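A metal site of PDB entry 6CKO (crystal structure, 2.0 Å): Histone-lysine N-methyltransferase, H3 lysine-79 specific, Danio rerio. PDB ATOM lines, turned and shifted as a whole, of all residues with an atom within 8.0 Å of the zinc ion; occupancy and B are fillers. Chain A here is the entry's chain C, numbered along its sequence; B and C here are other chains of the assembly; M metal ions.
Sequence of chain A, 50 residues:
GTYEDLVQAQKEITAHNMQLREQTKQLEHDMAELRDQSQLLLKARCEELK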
ATOM      1  N   GLN A  26      16.004  21.237  28.575  1.00  0.00           N
ATOM      2  CA  GLN A  26      17.305  20.628  28.888  1.00  0.00           C
ATOM      3  C   GLN A  26      17.347  20.181  30.323  1.00  0.00           C
ATOM      4  O   GLN A  26      17.826  19.083  30.619  1.00  0.00           O
ATOM      5  CB  GLN A  26      18.463  21.608  28.567  1.00  0.00           C
ATOM      6  CG  GLN A  26      18.557  21.875  27.031  1.00  0.00           C
ATOM      7  CD  GLN A  26      19.516  23.031  26.725  1.00  0.00           C
ATOM      8  OE1 GLN A  26      19.731  23.918  27.550  1.00  0.00           O
ATOM      9  NE2 GLN A  26      20.121  22.979  25.594  1.00  0.00           N
ATOM     10  N   HIS A  29      15.359  17.153  31.042  1.00  0.00           N
ATOM     11  CA  HIS A  29      16.133  16.000  30.713  1.00  0.00           C
ATOM     12  C   HIS A  29      17.240  15.725  31.753  1.00  0.00           C
ATOM     13  O   HIS A  29      17.454  14.550  32.146  1.00  0.00           O
ATOM     14  CB  HIS A  29      16.764  16.034  29.297  1.00  0.00           C
ATOM     15  CG  HIS A  29      17.427  14.743  28.937  1.00  0.00           C
ATOM     16  ND1 HIS A  29      16.701  13.625  28.599  1.00  0.00           N
ATOM     17  CD2 HIS A  29      18.741  14.360  28.930  1.00  0.00           C
ATOM     18  CE1 HIS A  29      17.537  12.615  28.353  1.00  0.00           C
ATOM     19  NE2 HIS A  29      18.766  13.046  28.531  1.00  0.00           N
ATOM     20  N   ASP A  30      17.925  16.783  32.186  1.00  0.00           N
ATOM     21  CA  ASP A  30      18.941  16.645  33.221  1.00  0.00           C
ATOM     22  C   ASP A  30      18.331  15.943  34.433  1.00  0.00           C
ATOM     23  O   ASP A  30      18.991  15.057  35.006  1.00  0.00           O
ATOM     24  CB  ASP A  30      19.513  17.963  33.721  1.00  0.00           C
ATOM     25  CG  ASP A  30      20.338  18.703  32.698  1.00  0.00           C
ATOM     26  OD1 ASP A  30      21.033  18.115  31.857  1.00  0.00           O
ATOM     27  OD2 ASP A  30      20.302  19.939  32.780  1.00  0.00           O
ATOM     28  N   ALA A  32      15.696  13.817  34.629  1.00  0.00           N
ATOM     29  CA  ALA A  32      15.428  12.407  34.339  1.00  0.00           C
ATOM     30  C   ALA A  32      16.686  11.568  34.410  1.00  0.00           C
ATOM     31  O   ALA A  32      16.661  10.472  35.002  1.00  0.00           O
ATOM     32  CB  ALA A  32      14.720  12.242  32.982  1.00  0.00           C
ATOM     33  N   GLU A  33      17.788  12.105  33.897  1.00  0.00           N
ATOM     34  CA  GLU A  33      19.095  11.443  33.983  1.00  0.00           C
ATOM     35  C   GLU A  33      19.519  11.316  35.461  1.00  0.00           C
ATOM     36  O   GLU A  33      19.992  10.269  35.917  1.00  0.00           O
ATOM     37  CB  GLU A  33      20.166  12.218  33.175  1.00  0.00           C
ATOM     38  CG  GLU A  33      20.022  12.106  31.622  1.00  0.00           C
ATOM     39  CD  GLU A  33      20.597  10.822  31.040  1.00  0.00           C
ATOM     40  OE1 GLU A  33      21.183  10.064  31.816  1.00  0.00           O
ATOM     41  OE2 GLU A  33      20.532  10.584  29.795  1.00  0.00           O
ATOM     42  N   LEU A  34      19.371  12.411  36.199  1.00  0.00           N
ATOM     43  CA  LEU A  34      19.798  12.428  37.580  1.00  0.00           C
ATOM     44  C   LEU A  34      19.009  11.464  38.466  1.00  0.00           C
ATOM     45  O   LEU A  34      19.599  10.762  39.264  1.00  0.00           O
ATOM     46  CB  LEU A  34      19.840  13.859  38.152  1.00  0.00           C
ATOM     47  CG  LEU A  34      21.006  14.699  37.607  1.00  0.00           C
ATOM     48  CD1 LEU A  34      20.797  16.188  37.824  1.00  0.00           C
ATOM     49  CD2 LEU A  34      22.334  14.235  38.174  1.00  0.00           C
ATOM     50  N   GLU B  22      16.038  13.085  18.305  1.00  0.00           N
ATOM     51  CA  GLU B  22      15.865  13.801  19.580  1.00  0.00           C
ATOM     52  C   GLU B  22      16.852  13.391  20.662  1.00  0.00           C
ATOM     53  O   GLU B  22      17.422  14.228  21.361  1.00  0.00           O
ATOM     54  CB  GLU B  22      14.434  13.622  20.086  1.00  0.00           C
ATOM     55  CG  GLU B  22      14.186  14.443  21.344  1.00  0.00           C
ATOM     56  N   GLN B  23      17.113  12.086  20.765  1.00  0.00           N
ATOM     57  CA  GLN B  23      18.048  11.584  21.725  1.00  0.00           C
ATOM     58  C   GLN B  23      19.500  12.065  21.483  1.00  0.00           C
ATOM     59  O   GLN B  23      20.284  12.217  22.421  1.00  0.00           O
ATOM     60  CB  GLN B  23      17.951  10.076  21.767  1.00  0.00           C
ATOM     61  CG  GLN B  23      18.677   9.544  22.949  1.00  0.00           C
ATOM     62  CD  GLN B  23      18.724   8.042  23.084  1.00  0.00           C
ATOM     63  OE1 GLN B  23      18.381   7.287  22.187  1.00  0.00           O
ATOM     64  NE2 GLN B  23      19.164   7.603  24.267  1.00  0.00           N
ATOM     65  N   THR B  24      19.856  12.306  20.216  1.00  0.00           N
ATOM     66  CA  THR B  24      21.145  12.857  19.888  1.00  0.00           C
ATOM     67  C   THR B  24      21.326  14.225  20.580  1.00  0.00           C
ATOM     68  O   THR B  24      22.367  14.507  21.161  1.00  0.00           O
ATOM     69  CB  THR B  24      21.286  12.950  18.332  1.00  0.00           C
ATOM     70  OG1 THR B  24      21.375  11.634  17.818  1.00  0.00           O
ATOM     71  CG2 THR B  24      22.535  13.721  17.932  1.00  0.00           C
ATOM     72  N   LYS B  25      20.319  15.067  20.496  1.00  0.00           N
ATOM     73  CA  LYS B  25      20.362  16.371  21.104  1.00  0.00           C
ATOM     74  C   LYS B  25      20.447  16.260  22.629  1.00  0.00           C
ATOM     75  O   LYS B  25      21.152  17.052  23.275  1.00  0.00           O
ATOM     76  CB  LYS B  25      19.129  17.189  20.715  1.00  0.00           C
ATOM     77  CG  LYS B  25      19.052  17.561  19.233  1.00  0.00           C
ATOM     78  CD  LYS B  25      17.685  18.148  18.933  1.00  0.00           C
ATOM     79  N   GLN B  26      19.732  15.296  23.196  1.00  0.00           N
ATOM     80  CA  GLN B  26      19.734  15.115  24.660  1.00  0.00           C
ATOM     81  C   GLN B  26      21.106  14.721  25.134  1.00  0.00           C
ATOM     82  O   GLN B  26      21.592  15.245  26.140  1.00  0.00           O
ATOM     83  CB  GLN B  26      18.673  14.082  25.096  1.00  0.00           C
ATOM     84  CG  GLN B  26      17.233  14.616  24.814  1.00  0.00           C
ATOM     85  CD  GLN B  26      16.185  13.513  24.999  1.00  0.00           C
ATOM     86  OE1 GLN B  26      16.474  12.325  24.855  1.00  0.00           O
ATOM     87  NE2 GLN B  26      15.020  13.908  25.375  1.00  0.00           N
ATOM     88  N   LEU B  27      21.680  13.737  24.433  1.00  0.00           N
ATOM     89  CA  LEU B  27      22.998  13.223  24.735  1.00  0.00           C
ATOM     90  C   LEU B  27      24.102  14.290  24.559  1.00  0.00           C
ATOM     91  O   LEU B  27      25.052  14.324  25.336  1.00  0.00           O
ATOM     92  CB  LEU B  27      23.298  11.953  23.901  1.00  0.00           C
ATOM     93  CG  LEU B  27      22.745  10.594  24.319  1.00  0.00           C
ATOM     94  CD1 LEU B  27      22.776   9.591  23.154  1.00  0.00           C
ATOM     95  CD2 LEU B  27      23.473  10.003  25.486  1.00  0.00           C
ATOM     96  N   GLU B  28      23.964  15.147  23.547  1.00  0.00           N
ATOM     97  CA  GLU B  28      24.859  16.289  23.375  1.00  0.00           C
ATOM     98  C   GLU B  28      24.810  17.210  24.582  1.00  0.00           C
ATOM     99  O   GLU B  28      25.870  17.690  25.052  1.00  0.00           O
ATOM    100  CB  GLU B  28      24.617  17.028  22.071  1.00  0.00           C
ATOM    101  CG  GLU B  28      25.025  16.097  20.896  1.00  0.00           C
ATOM    102  CD  GLU B  28      24.618  16.595  19.556  1.00  0.00           C
ATOM    103  OE1 GLU B  28      23.765  17.493  19.461  1.00  0.00           O
ATOM    104  OE2 GLU B  28      25.183  16.102  18.590  1.00  0.00           O
ATOM    105  N   HIS B  29      23.596  17.455  25.075  1.00  0.00           N
ATOM    106  CA  HIS B  29      23.455  18.237  26.276  1.00  0.00           C
ATOM    107  C   HIS B  29      24.038  17.502  27.501  1.00  0.00           C
ATOM    108  O   HIS B  29      24.734  18.146  28.337  1.00  0.00           O
ATOM    109  CB  HIS B  29      22.011  18.681  26.577  1.00  0.00           C
ATOM    110  CG  HIS B  29      21.942  19.618  27.741  1.00  0.00           C
ATOM    111  ND1 HIS B  29      22.345  20.940  27.642  1.00  0.00           N
ATOM    112  CD2 HIS B  29      21.593  19.428  29.050  1.00  0.00           C
ATOM    113  CE1 HIS B  29      22.202  21.526  28.824  1.00  0.00           C
ATOM    114  NE2 HIS B  29      21.729  20.641  29.683  1.00  0.00           N
ATOM    115  N   ASP B  30      23.756  16.204  27.612  1.00  0.00           N
ATOM    116  CA  ASP B  30      24.311  15.407  28.698  1.00  0.00           C
ATOM    117  C   ASP B  30      25.830  15.568  28.714  1.00  0.00           C
ATOM    118  O   ASP B  30      26.404  15.720  29.807  1.00  0.00           O
ATOM    119  CB  ASP B  30      24.030  13.916  28.593  1.00  0.00           C
ATOM    120  CG  ASP B  30      22.578  13.549  28.768  1.00  0.00           C
ATOM    121  OD1 ASP B  30      21.828  14.180  29.535  1.00  0.00           O
ATOM    122  OD2 ASP B  30      22.190  12.560  28.130  1.00  0.00           O
ATOM    123  N   MET B  31      26.474  15.484  27.553  1.00  0.00           N
ATOM    124  CA  MET B  31      27.918  15.679  27.467  1.00  0.00           C
ATOM    125  C   MET B  31      28.469  17.036  27.921  1.00  0.00           C
ATOM    126  O   MET B  31      29.535  17.092  28.569  1.00  0.00           O
ATOM    127  CB  MET B  31      28.429  15.402  26.042  1.00  0.00           C
ATOM    128  CG  MET B  31      29.574  14.426  26.045  1.00  0.00           C
ATOM    129  SD  MET B  31      29.115  12.749  26.504  1.00  0.00           S
ATOM    130  CE  MET B  31      28.026  12.329  25.172  1.00  0.00           C
ATOM    131  N   LEU B  34      28.268  17.031  31.645  1.00  0.00           N
ATOM    132  CA  LEU B  34      29.278  16.160  32.203  1.00  0.00           C
ATOM    133  C   LEU B  34      30.676  16.757  32.156  1.00  0.00           C
ATOM    134  O   LEU B  34      31.406  16.677  33.125  1.00  0.00           O
ATOM    135  CB  LEU B  34      29.213  14.743  31.600  1.00  0.00           C
ATOM    136  CG  LEU B  34      28.002  13.929  32.085  1.00  0.00           C
ATOM    137  CD1 LEU B  34      27.707  12.740  31.187  1.00  0.00           C
ATOM    138  CD2 LEU B  34      28.166  13.505  33.533  1.00  0.00           C
ATOM    139  N   THR C  63      26.471   7.559  23.813  1.00  0.00           N
ATOM    140  CA  THR C  63      26.136   6.772  25.008  1.00  0.00           C
ATOM    141  C   THR C  63      27.360   6.279  25.719  1.00  0.00           C
ATOM    142  O   THR C  63      27.454   6.482  26.953  1.00  0.00           O
ATOM    143  CB  THR C  63      25.134   5.656  24.717  1.00  0.00           C
ATOM    144  OG1 THR C  63      23.966   6.267  24.148  1.00  0.00           O
ATOM    145  CG2 THR C  63      24.737   4.869  25.998  1.00  0.00           C
ATOM    146  N   LYS C  66      29.192   9.288  27.391  1.00  0.00           N
ATOM    147  CA  LYS C  66      28.388   9.675  28.539  1.00  0.00           C
ATOM    148  C   LYS C  66      28.653   8.769  29.739  1.00  0.00           C
ATOM    149  O   LYS C  66      28.923   9.254  30.823  1.00  0.00           O
ATOM    150  CB  LYS C  66      26.866   9.676  28.215  1.00  0.00           C
ATOM    151  CG  LYS C  66      25.916   9.823  29.419  1.00  0.00           C
ATOM    152  CD  LYS C  66      24.438   9.540  29.056  1.00  0.00           C
ATOM    153  CE  LYS C  66      23.620   9.274  30.270  1.00  0.00           C
ATOM    154  NZ  LYS C  66      22.421   8.435  30.049  1.00  0.00           N
ATOM    155  N   GLN C  70      30.382   9.761  33.292  1.00  0.00           N
ATOM    156  CA  GLN C  70      29.696   9.562  34.584  1.00  0.00           C
ATOM    157  C   GLN C  70      30.599   8.836  35.535  1.00  0.00           C
ATOM    158  O   GLN C  70      30.683   9.214  36.722  1.00  0.00           O
ATOM    159  CB  GLN C  70      28.355   8.800  34.423  1.00  0.00           C
ATOM    160  CG  GLN C  70      27.333   9.652  33.680  1.00  0.00           C
ATOM    161  CD  GLN C  70      26.022   8.951  33.392  1.00  0.00           C
ATOM    162  OE1 GLN C  70      25.986   7.844  32.944  1.00  0.00           O
ATOM    163  NE2 GLN C  70      24.924   9.619  33.655  1.00  0.00           N
HETATM  164 ZN    ZN M   1      20.390  11.886  28.375  1.00  0.00          ZN
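OE1 of Glu 33 is in salt-bridge range of NZ of Lys 66 of chain C (2.7 Å).
Three residues have an atom within 4 Å of the zinc ion: His 29 of chain A, Glu 33 and Asp 30 of chain B.
The nearest printed residue that does not touch the zinc ion is Gln 26 of chain B (4.2 Å).
The zinc ion is bound by OE2 of Glu 33 (1.9 Å), OD2 of Asp 30 of chain B (1.9 Å) and NE2 of His 29 of chain A (2.0 Å).
The zinc ion has three donor atoms within binding distance.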
